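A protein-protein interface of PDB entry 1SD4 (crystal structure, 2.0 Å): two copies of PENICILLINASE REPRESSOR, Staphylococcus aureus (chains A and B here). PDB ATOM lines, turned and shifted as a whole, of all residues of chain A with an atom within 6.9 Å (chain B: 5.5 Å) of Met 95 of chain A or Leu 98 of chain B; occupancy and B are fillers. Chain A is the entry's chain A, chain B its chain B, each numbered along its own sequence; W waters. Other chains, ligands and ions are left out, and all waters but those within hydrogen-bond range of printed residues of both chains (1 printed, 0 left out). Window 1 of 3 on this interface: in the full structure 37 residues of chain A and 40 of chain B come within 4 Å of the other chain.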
ATOM      1  N   MET A  80      30.738 -24.101 -10.838  1.00  0.00           N
ATOM      2  CA  MET A  80      30.564 -25.532 -10.618  1.00  0.00           C
ATOM      3  C   MET A  80      30.855 -25.846  -9.144  1.00  0.00           C
ATOM      4  O   MET A  80      30.100 -26.549  -8.491  1.00  0.00           O
ATOM      5  CB  MET A  80      31.495 -26.335 -11.523  1.00  0.00           C
ATOM      6  CG  MET A  80      31.211 -27.809 -11.568  1.00  0.00           C
ATOM      7  SD  MET A  80      29.387 -28.213 -12.165  1.00  0.00           S
ATOM      8  CE  MET A  80      28.763 -28.949 -10.543  1.00  0.00           C
ATOM      9  N   ALA A  83      27.966 -24.439  -7.040  1.00  0.00           N
ATOM     10  CA  ALA A  83      26.748 -25.184  -7.269  1.00  0.00           C
ATOM     11  C   ALA A  83      26.838 -26.536  -6.624  1.00  0.00           C
ATOM     12  O   ALA A  83      25.850 -27.039  -6.090  1.00  0.00           O
ATOM     13  CB  ALA A  83      26.511 -25.322  -8.772  1.00  0.00           C
ATOM     14  N   PHE A  86      26.230 -26.244  -3.015  1.00  0.00           N
ATOM     15  CA  PHE A  86      24.798 -25.950  -2.860  1.00  0.00           C
ATOM     16  C   PHE A  86      23.930 -27.228  -2.903  1.00  0.00           C
ATOM     17  O   PHE A  86      23.133 -27.488  -1.999  1.00  0.00           O
ATOM     18  CB  PHE A  86      24.359 -25.031  -3.996  1.00  0.00           C
ATOM     19  CG  PHE A  86      22.896 -24.700  -3.972  1.00  0.00           C
ATOM     20  CD1 PHE A  86      22.403 -23.803  -3.027  1.00  0.00           C
ATOM     21  CD2 PHE A  86      22.015 -25.273  -4.891  1.00  0.00           C
ATOM     22  CE1 PHE A  86      21.042 -23.494  -2.973  1.00  0.00           C
ATOM     23  CE2 PHE A  86      20.613 -24.975  -4.852  1.00  0.00           C
ATOM     24  CZ  PHE A  86      20.148 -24.079  -3.897  1.00  0.00           C
ATOM     25  N   LEU A  87      24.105 -28.000  -3.968  1.00  0.00           N
ATOM     26  CA  LEU A  87      23.355 -29.247  -4.175  1.00  0.00           C
ATOM     27  C   LEU A  87      23.592 -30.230  -3.042  1.00  0.00           C
ATOM     28  O   LEU A  87      22.642 -30.824  -2.487  1.00  0.00           O
ATOM     29  CB  LEU A  87      23.666 -29.839  -5.572  1.00  0.00           C
ATOM     30  CG  LEU A  87      22.680 -30.888  -6.126  1.00  0.00           C
ATOM     31  CD1 LEU A  87      21.314 -30.307  -6.460  1.00  0.00           C
ATOM     32  CD2 LEU A  87      23.309 -31.596  -7.324  1.00  0.00           C
ATOM     33  N   TYR A  91      20.206 -30.431  -1.072  1.00  0.00           N
ATOM     34  CA  TYR A  91      19.475 -31.477  -1.798  1.00  0.00           C
ATOM     35  C   TYR A  91      20.185 -32.818  -1.744  1.00  0.00           C
ATOM     36  O   TYR A  91      20.031 -33.621  -2.660  1.00  0.00           O
ATOM     37  CB  TYR A  91      19.177 -31.056  -3.251  1.00  0.00           C
ATOM     38  CG  TYR A  91      18.210 -29.876  -3.296  1.00  0.00           C
ATOM     39  CD1 TYR A  91      16.830 -30.058  -3.090  1.00  0.00           C
ATOM     40  CD2 TYR A  91      18.677 -28.588  -3.487  1.00  0.00           C
ATOM     41  CE1 TYR A  91      15.936 -28.971  -3.087  1.00  0.00           C
ATOM     42  CE2 TYR A  91      17.806 -27.487  -3.497  1.00  0.00           C
ATOM     43  CZ  TYR A  91      16.429 -27.692  -3.287  1.00  0.00           C
ATOM     44  OH  TYR A  91      15.557 -26.622  -3.305  1.00  0.00           O
ATOM     45  N   GLY A  92      20.966 -33.047  -0.703  1.00  0.00           N
ATOM     46  CA  GLY A  92      21.644 -34.335  -0.512  1.00  0.00           C
ATOM     47  C   GLY A  92      22.516 -34.695  -1.719  1.00  0.00           C
ATOM     48  O   GLY A  92      22.829 -35.868  -1.944  1.00  0.00           O
ATOM     49  N   GLY A  93      22.863 -33.684  -2.521  1.00  0.00           N
ATOM     50  CA  GLY A  93      23.685 -33.863  -3.706  1.00  0.00           C
ATOM     51  C   GLY A  93      22.930 -34.504  -4.859  1.00  0.00           C
ATOM     52  O   GLY A  93      23.561 -35.037  -5.791  1.00  0.00           O
ATOM     53  N   ASP A  94      21.596 -34.468  -4.816  1.00  0.00           N
ATOM     54  CA  ASP A  94      20.773 -35.116  -5.844  1.00  0.00           C
ATOM     55  C   ASP A  94      20.103 -34.072  -6.737  1.00  0.00           C
ATOM     56  O   ASP A  94      19.255 -33.283  -6.259  1.00  0.00           O
ATOM     57  CB  ASP A  94      19.686 -35.987  -5.195  1.00  0.00           C
ATOM     58  CG  ASP A  94      20.220 -37.297  -4.651  1.00  0.00           C
ATOM     59  OD1 ASP A  94      21.134 -37.899  -5.287  1.00  0.00           O
ATOM     60  OD2 ASP A  94      19.782 -37.796  -3.579  1.00  0.00           O
ATOM     61  N   MET A  95      20.472 -34.069  -8.014  1.00  0.00           N
ATOM     62  CA  MET A  95      19.810 -33.190  -8.987  1.00  0.00           C
ATOM     63  C   MET A  95      18.293 -33.386  -9.031  1.00  0.00           C
ATOM     64  O   MET A  95      17.544 -32.417  -9.043  1.00  0.00           O
ATOM     65  CB  MET A  95      20.388 -33.372 -10.380  1.00  0.00           C
ATOM     66  CG  MET A  95      19.827 -32.378 -11.426  1.00  0.00           C
ATOM     67  SD  MET A  95      20.335 -30.529 -10.972  1.00  0.00           S
ATOM     68  CE  MET A  95      22.233 -30.680 -11.480  1.00  0.00           C
ATOM     69  N   LYS A  96      17.837 -34.633  -9.045  1.00  0.00           N
ATOM     70  CA  LYS A  96      16.390 -34.916  -9.067  1.00  0.00           C
ATOM     71  C   LYS A  96      15.622 -34.292  -7.890  1.00  0.00           C
ATOM     72  O   LYS A  96      14.472 -33.909  -8.028  1.00  0.00           O
ATOM     73  CB  LYS A  96      16.143 -36.417  -9.094  1.00  0.00           C
ATOM     74  CG  LYS A  96      16.723 -37.160  -7.901  1.00  0.00           C
ATOM     75  CD  LYS A  96      16.495 -38.673  -8.022  1.00  0.00           C
ATOM     76  CE  LYS A  96      17.219 -39.398  -6.921  1.00  0.00           C
ATOM     77  NZ  LYS A  96      16.994 -40.872  -7.036  1.00  0.00           N
ATOM     78  N   SER A  97      16.275 -34.199  -6.735  1.00  0.00           N
ATOM     79  CA  SER A  97      15.646 -33.646  -5.553  1.00  0.00           C
ATOM     80  C   SER A  97      15.402 -32.154  -5.751  1.00  0.00           C
ATOM     81  O   SER A  97      14.326 -31.641  -5.424  1.00  0.00           O
ATOM     82  CB  SER A  97      16.508 -33.931  -4.300  1.00  0.00           C
ATOM     83  OG  SER A  97      15.930 -33.305  -3.155  1.00  0.00           O
ATOM     84  N   LEU A  98      16.383 -31.458  -6.309  1.00  0.00           N
ATOM     85  CA  LEU A  98      16.239 -30.035  -6.620  1.00  0.00           C
ATOM     86  C   LEU A  98      15.163 -29.809  -7.720  1.00  0.00           C
ATOM     87  O   LEU A  98      14.249 -28.945  -7.575  1.00  0.00           O
ATOM     88  CB  LEU A  98      17.593 -29.470  -7.077  1.00  0.00           C
ATOM     89  CG  LEU A  98      17.631 -28.098  -7.742  1.00  0.00           C
ATOM     90  CD1 LEU A  98      17.051 -27.095  -6.800  1.00  0.00           C
ATOM     91  CD2 LEU A  98      19.117 -27.745  -8.016  1.00  0.00           C
ATOM     92  N   VAL A  99      15.257 -30.587  -8.791  1.00  0.00           N
ATOM     93  CA  VAL A  99      14.300 -30.412  -9.884  1.00  0.00           C
ATOM     94  C   VAL A  99      12.876 -30.689  -9.398  1.00  0.00           C
ATOM     95  O   VAL A  99      11.918 -29.960  -9.763  1.00  0.00           O
ATOM     96  CB  VAL A  99      14.659 -31.277 -11.136  1.00  0.00           C
ATOM     97  CG1 VAL A  99      13.548 -31.150 -12.221  1.00  0.00           C
ATOM     98  CG2 VAL A  99      16.010 -30.860 -11.723  1.00  0.00           C
ATOM     99  N   LEU A 100      12.722 -31.714  -8.547  1.00  0.00           N
ATOM    100  CA  LEU A 100      11.408 -32.035  -8.013  1.00  0.00           C
ATOM    101  C   LEU A 100      10.878 -30.990  -7.063  1.00  0.00           C
ATOM    102  O   LEU A 100       9.681 -30.677  -7.094  1.00  0.00           O
ATOM    103  CB  LEU A 100      11.373 -33.418  -7.323  1.00  0.00           C
ATOM    104  CG  LEU A 100      11.311 -34.540  -8.335  1.00  0.00           C
ATOM    105  CD1 LEU A 100      11.652 -35.883  -7.667  1.00  0.00           C
ATOM    106  CD2 LEU A 100       9.905 -34.573  -8.959  1.00  0.00           C
ATOM    107  N   ASN A 101      11.737 -30.465  -6.208  1.00  0.00           N
ATOM    108  CA  ASN A 101      11.337 -29.400  -5.310  1.00  0.00           C
ATOM    109  C   ASN A 101      10.748 -28.236  -6.132  1.00  0.00           C
ATOM    110  O   ASN A 101       9.758 -27.608  -5.710  1.00  0.00           O
ATOM    111  CB  ASN A 101      12.534 -28.943  -4.504  1.00  0.00           C
ATOM    112  CG  ASN A 101      12.154 -28.107  -3.317  1.00  0.00           C
ATOM    113  OD1 ASN A 101      11.135 -28.369  -2.660  1.00  0.00           O
ATOM    114  ND2 ASN A 101      12.985 -27.090  -3.010  1.00  0.00           N
ATOM    115  N   PHE B  86      19.813 -18.822  -6.147  1.00  0.00           N
ATOM    116  CA  PHE B  86      20.948 -19.517  -6.683  1.00  0.00           C
ATOM    117  C   PHE B  86      20.779 -19.724  -8.204  1.00  0.00           C
ATOM    118  O   PHE B  86      21.684 -19.409  -8.983  1.00  0.00           O
ATOM    119  CB  PHE B  86      21.041 -20.841  -5.954  1.00  0.00           C
ATOM    120  CG  PHE B  86      22.129 -21.702  -6.408  1.00  0.00           C
ATOM    121  CD1 PHE B  86      23.405 -21.521  -5.901  1.00  0.00           C
ATOM    122  CD2 PHE B  86      21.895 -22.715  -7.337  1.00  0.00           C
ATOM    123  CE1 PHE B  86      24.453 -22.323  -6.324  1.00  0.00           C
ATOM    124  CE2 PHE B  86      22.964 -23.545  -7.777  1.00  0.00           C
ATOM    125  CZ  PHE B  86      24.230 -23.330  -7.266  1.00  0.00           C
ATOM    126  N   LEU B  87      19.623 -20.237  -8.629  1.00  0.00           N
ATOM    127  CA  LEU B  87      19.359 -20.455 -10.066  1.00  0.00           C
ATOM    128  C   LEU B  87      19.413 -19.109 -10.832  1.00  0.00           C
ATOM    129  O   LEU B  87      19.979 -18.997 -11.924  1.00  0.00           O
ATOM    130  CB  LEU B  87      17.996 -21.121 -10.266  1.00  0.00           C
ATOM    131  CG  LEU B  87      17.669 -21.642 -11.662  1.00  0.00           C
ATOM    132  CD1 LEU B  87      18.574 -22.886 -12.010  1.00  0.00           C
ATOM    133  CD2 LEU B  87      16.187 -21.975 -11.753  1.00  0.00           C
ATOM    134  N   TYR B  91      22.713 -19.192 -12.986  1.00  0.00           N
ATOM    135  CA  TYR B  91      22.239 -19.833 -14.220  1.00  0.00           C
ATOM    136  C   TYR B  91      21.164 -19.063 -14.960  1.00  0.00           C
ATOM    137  O   TYR B  91      20.418 -19.653 -15.720  1.00  0.00           O
ATOM    138  CB  TYR B  91      21.744 -21.301 -13.969  1.00  0.00           C
ATOM    139  CG  TYR B  91      22.859 -22.155 -13.365  1.00  0.00           C
ATOM    140  CD1 TYR B  91      23.933 -22.618 -14.163  1.00  0.00           C
ATOM    141  CD2 TYR B  91      22.890 -22.417 -11.992  1.00  0.00           C
ATOM    142  CE1 TYR B  91      24.976 -23.378 -13.607  1.00  0.00           C
ATOM    143  CE2 TYR B  91      23.928 -23.153 -11.417  1.00  0.00           C
ATOM    144  CZ  TYR B  91      24.974 -23.622 -12.238  1.00  0.00           C
ATOM    145  OH  TYR B  91      25.992 -24.366 -11.687  1.00  0.00           O
ATOM    146  N   ASP B  94      17.495 -20.297 -15.347  1.00  0.00           N
ATOM    147  CA  ASP B  94      17.204 -21.344 -16.335  1.00  0.00           C
ATOM    148  C   ASP B  94      17.655 -22.709 -15.814  1.00  0.00           C
ATOM    149  O   ASP B  94      18.842 -22.974 -15.704  1.00  0.00           O
ATOM    150  CB  ASP B  94      17.932 -20.983 -17.645  1.00  0.00           C
ATOM    151  CG  ASP B  94      17.464 -21.794 -18.836  1.00  0.00           C
ATOM    152  OD1 ASP B  94      16.786 -22.854 -18.675  1.00  0.00           O
ATOM    153  OD2 ASP B  94      17.757 -21.453 -20.002  1.00  0.00           O
ATOM    154  N   MET B  95      16.702 -23.545 -15.412  1.00  0.00           N
ATOM    155  CA  MET B  95      17.018 -24.906 -14.929  1.00  0.00           C
ATOM    156  C   MET B  95      17.787 -25.712 -15.965  1.00  0.00           C
ATOM    157  O   MET B  95      18.637 -26.551 -15.632  1.00  0.00           O
ATOM    158  CB  MET B  95      15.733 -25.632 -14.523  1.00  0.00           C
ATOM    159  CG  MET B  95      15.929 -26.972 -13.830  1.00  0.00           C
ATOM    160  SD  MET B  95      16.847 -26.829 -12.111  1.00  0.00           S
ATOM    161  CE  MET B  95      15.321 -26.063 -11.146  1.00  0.00           C
ATOM    162  N   LYS B  96      17.518 -25.455 -17.241  1.00  0.00           N
ATOM    163  CA  LYS B  96      18.187 -26.231 -18.298  1.00  0.00           C
ATOM    164  C   LYS B  96      19.678 -25.906 -18.318  1.00  0.00           C
ATOM    165  O   LYS B  96      20.510 -26.747 -18.675  1.00  0.00           O
ATOM    166  CB  LYS B  96      17.542 -25.945 -19.680  1.00  0.00           C
ATOM    167  CG  LYS B  96      18.176 -24.761 -20.429  1.00  0.00           C
ATOM    168  CD  LYS B  96      17.470 -24.470 -21.782  1.00  0.00           C
ATOM    169  CE  LYS B  96      16.182 -23.662 -21.579  1.00  0.00           C
ATOM    170  NZ  LYS B  96      15.979 -22.643 -22.626  1.00  0.00           N
ATOM    171  N   SER B  97      20.025 -24.690 -17.892  1.00  0.00           N
ATOM    172  CA  SER B  97      21.425 -24.262 -17.848  1.00  0.00           C
ATOM    173  C   SER B  97      22.142 -24.911 -16.666  1.00  0.00           C
ATOM    174  O   SER B  97      23.270 -25.406 -16.807  1.00  0.00           O
ATOM    175  CB  SER B  97      21.513 -22.740 -17.786  1.00  0.00           C
ATOM    176  OG  SER B  97      22.868 -22.324 -17.671  1.00  0.00           O
ATOM    177  N   LEU B  98      21.470 -24.995 -15.526  1.00  0.00           N
ATOM    178  CA  LEU B  98      22.051 -25.736 -14.392  1.00  0.00           C
ATOM    179  C   LEU B  98      22.323 -27.165 -14.779  1.00  0.00           C
ATOM    180  O   LEU B  98      23.414 -27.678 -14.560  1.00  0.00           O
ATOM    181  CB  LEU B  98      21.130 -25.713 -13.153  1.00  0.00           C
ATOM    182  CG  LEU B  98      21.630 -26.274 -11.799  1.00  0.00           C
ATOM    183  CD1 LEU B  98      20.712 -25.835 -10.728  1.00  0.00           C
ATOM    184  CD2 LEU B  98      21.509 -27.701 -11.818  1.00  0.00           C
ATOM    185  N   VAL B  99      21.310 -27.830 -15.315  1.00  0.00           N
ATOM    186  CA  VAL B  99      21.493 -29.223 -15.718  1.00  0.00           C
ATOM    187  C   VAL B  99      22.626 -29.422 -16.752  1.00  0.00           C
ATOM    188  O   VAL B  99      23.426 -30.357 -16.617  1.00  0.00           O
ATOM    189  CB  VAL B  99      20.177 -29.833 -16.231  1.00  0.00           C
ATOM    190  CG1 VAL B  99      20.367 -31.296 -16.587  1.00  0.00           C
ATOM    191  CG2 VAL B  99      19.135 -29.734 -15.118  1.00  0.00           C
ATOM    192  N   LEU B 100      22.691 -28.584 -17.785  1.00  0.00           N
ATOM    193  CA  LEU B 100      23.723 -28.744 -18.826  1.00  0.00           C
ATOM    194  C   LEU B 100      25.121 -28.441 -18.288  1.00  0.00           C
ATOM    195  O   LEU B 100      26.103 -29.104 -18.657  1.00  0.00           O
ATOM    196  CB  LEU B 100      23.427 -27.849 -20.048  1.00  0.00           C
ATOM    197  CG  LEU B 100      22.271 -28.387 -20.957  1.00  0.00           C
ATOM    198  CD1 LEU B 100      21.911 -27.364 -22.052  1.00  0.00           C
ATOM    199  CD2 LEU B 100      22.611 -29.757 -21.564  1.00  0.00           C
ATOM    200  N   ASN B 101      25.213 -27.460 -17.391  1.00  0.00           N
ATOM    201  CA  ASN B 101      26.485 -27.139 -16.774  1.00  0.00           C
ATOM    202  C   ASN B 101      26.997 -28.307 -15.936  1.00  0.00           C
ATOM    203  O   ASN B 101      28.208 -28.578 -15.933  1.00  0.00           O
ATOM    204  CB  ASN B 101      26.378 -25.871 -15.928  1.00  0.00           C
ATOM    205  CG  ASN B 101      26.701 -24.602 -16.751  1.00  0.00           C
ATOM    206  OD1 ASN B 101      27.868 -24.264 -16.971  1.00  0.00           O
ATOM    207  ND2 ASN B 101      25.672 -23.954 -17.259  1.00  0.00           N
ATOM    208  N   PHE B 102      26.089 -29.024 -15.273  1.00  0.00           N
ATOM    209  CA  PHE B 102      26.494 -30.201 -14.485  1.00  0.00           C
ATOM    210  C   PHE B 102      26.912 -31.368 -15.390  1.00  0.00           C
ATOM    211  O   PHE B 102      27.909 -32.068 -15.136  1.00  0.00           O
ATOM    212  CB  PHE B 102      25.359 -30.648 -13.559  1.00  0.00           C
ATOM    213  CG  PHE B 102      25.405 -30.016 -12.223  1.00  0.00           C
ATOM    214  CD1 PHE B 102      25.259 -28.626 -12.088  1.00  0.00           C
ATOM    215  CD2 PHE B 102      25.595 -30.804 -11.082  1.00  0.00           C
ATOM    216  CE1 PHE B 102      25.302 -28.011 -10.823  1.00  0.00           C
ATOM    217  CE2 PHE B 102      25.635 -30.216  -9.812  1.00  0.00           C
ATOM    218  CZ  PHE B 102      25.486 -28.807  -9.670  1.00  0.00           C
ATOM    219  N   ALA B 103      26.127 -31.587 -16.433  1.00  0.00           N
ATOM    220  CA  ALA B 103      26.414 -32.674 -17.351  1.00  0.00           C
ATOM    221  C   ALA B 103      27.764 -32.506 -18.052  1.00  0.00           C
ATOM    222  O   ALA B 103      28.525 -33.464 -18.111  1.00  0.00           O
ATOM    223  CB  ALA B 103      25.293 -32.834 -18.364  1.00  0.00           C
ATOM    224  N   LEU B 108      26.965 -35.146 -13.410  1.00  0.00           N
ATOM    225  CA  LEU B 108      25.679 -35.800 -13.582  1.00  0.00           C
ATOM    226  C   LEU B 108      25.949 -36.915 -14.567  1.00  0.00           C
ATOM    227  O   LEU B 108      26.226 -36.654 -15.731  1.00  0.00           O
ATOM    228  CB  LEU B 108      24.657 -34.788 -14.132  1.00  0.00           C
ATOM    229  CG  LEU B 108      23.166 -35.035 -13.902  1.00  0.00           C
ATOM    230  CD1 LEU B 108      22.835 -35.009 -12.424  1.00  0.00           C
ATOM    231  CD2 LEU B 108      22.261 -34.084 -14.716  1.00  0.00           C
ATOM    232  N   LEU B 116      16.359 -38.713 -14.466  1.00  0.00           N
ATOM    233  CA  LEU B 116      15.735 -37.409 -14.473  1.00  0.00           C
ATOM    234  C   LEU B 116      14.820 -37.214 -15.693  1.00  0.00           C
ATOM    235  O   LEU B 116      13.709 -36.664 -15.593  1.00  0.00           O
ATOM    236  CB  LEU B 116      16.779 -36.315 -14.416  1.00  0.00           C
ATOM    237  CG  LEU B 116      16.173 -34.972 -14.030  1.00  0.00           C
ATOM    238  CD1 LEU B 116      15.334 -35.126 -12.761  1.00  0.00           C
ATOM    239  CD2 LEU B 116      17.284 -33.988 -13.828  1.00  0.00           C
HETATM  240  O   HOH W   1      28.038 -25.368 -13.004  1.00  0.00           O
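Met 95 of chain A touches four residues of chain B. Leu 98 of chain B touches two residues of chain A. Printed residues of chain A within 4 Å of Leu 116 of chain B: Met 95 (3.9 Å), Lys 96 (3.8 Å) and Val 99 (3.98 Å). Printed residues of chain A within 4 Å of Phe 102 of chain B: Met 80, Ala 83, Leu 87 and Met 95. Printed residues of chain A within 4 Å of Tyr 91 of chain B: Ala 83. Met 95 of chain B touches none of the printed residues of chain A. Asn 101 of chain A touches none of the printed residues of chain B. The nearest residue of chain B that does not touch Met 95 of chain A is Val 99 of chain B (4.4 Å). The nearest residue of chain A that does not touch Leu 98 of chain B is Ala 83 of chain A (5.8 Å).
Water W1 lies within hydrogen-bond range of the side-chain hydroxyl (OH) of Tyr 91 of chain B (2.6 Å) and the side-chain sulfur (SD) of Met 80 of chain A (3.3 Å).
Hydrophobic or aromatic side chains of chain B that line the printed part of chain A: Phe 86, Tyr 91, Leu 98, Phe 102, Leu 108 and Leu 116. Of the 15 printed residues of chain A, 8 touch a printed residue of chain B. Hydrophobic or aromatic side chains of chain A that line the printed part of chain B: Met 80, Ala 83, Phe 86, Leu 87, Met 95, Leu 98 and Val 99.
N of Gly 92 of chain A is in hydrogen-bond range of O of Leu 87 of chain A (3.3 Å). O of Leu 87 of chain A lies within hydrogen-bond range of N of Gly 93 of chain A (2.9 Å). The side-chain amide nitrogen (ND2) of Asn 101 of chain B lies within hydrogen-bond range of the backbone carbonyl oxygen (O) of Ser 97 of chain B, 2.8 Å away.
Phe 86 of chain A touches its own counterpart, Phe 86 of chain B. Met 95 of chain A touches Leu 98 of chain B, but with the chains exchanged Leu 98 of chain A does not touch Met 95 of chain B (4.6 Å). Leu 98 of chain A touches its own counterpart, Leu 98 of chain B. Positions printed for both chains: 86, 87, 91, 94, 95, 96, 97, 98, 99, 100 and 101. Of the 14 pairs that touch across the chains among the printed residues, 2 have their exchanged pair printed and touching as well.
SD of Met 80 of chain A touches O of Asn 101 of chain B, 3.96 Å away. Phe 102 of chain B touches Met 80 of chain A (CZ to CE, 3.4 Å). CZ of Phe 86 of chain B touches CA of Ala 83 of chain A, at 3.1 Å. Ala 83 of chain A touches Phe 102 of chain B (CB to CE1, 3.6 Å). Phe 86 of chain B touches Phe 86 of chain A (CE2 to CD2, 3.5 Å). Leu 98 of chain B touches Met 95 of chain A (CD2 to CE, 3.1 Å). CD1 of Leu 108 of chain B touches CB of Met 95 of chain A, 3.6 Å away. Lys 96 of chain A touches Leu 116 of chain B (CA to CD1, 3.8 Å). Leu 98 of chain B touches Leu 98 of chain A (CD1 to CD2, 3.7 Å). Leu 116 of chain B touches Val 99 of chain A.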
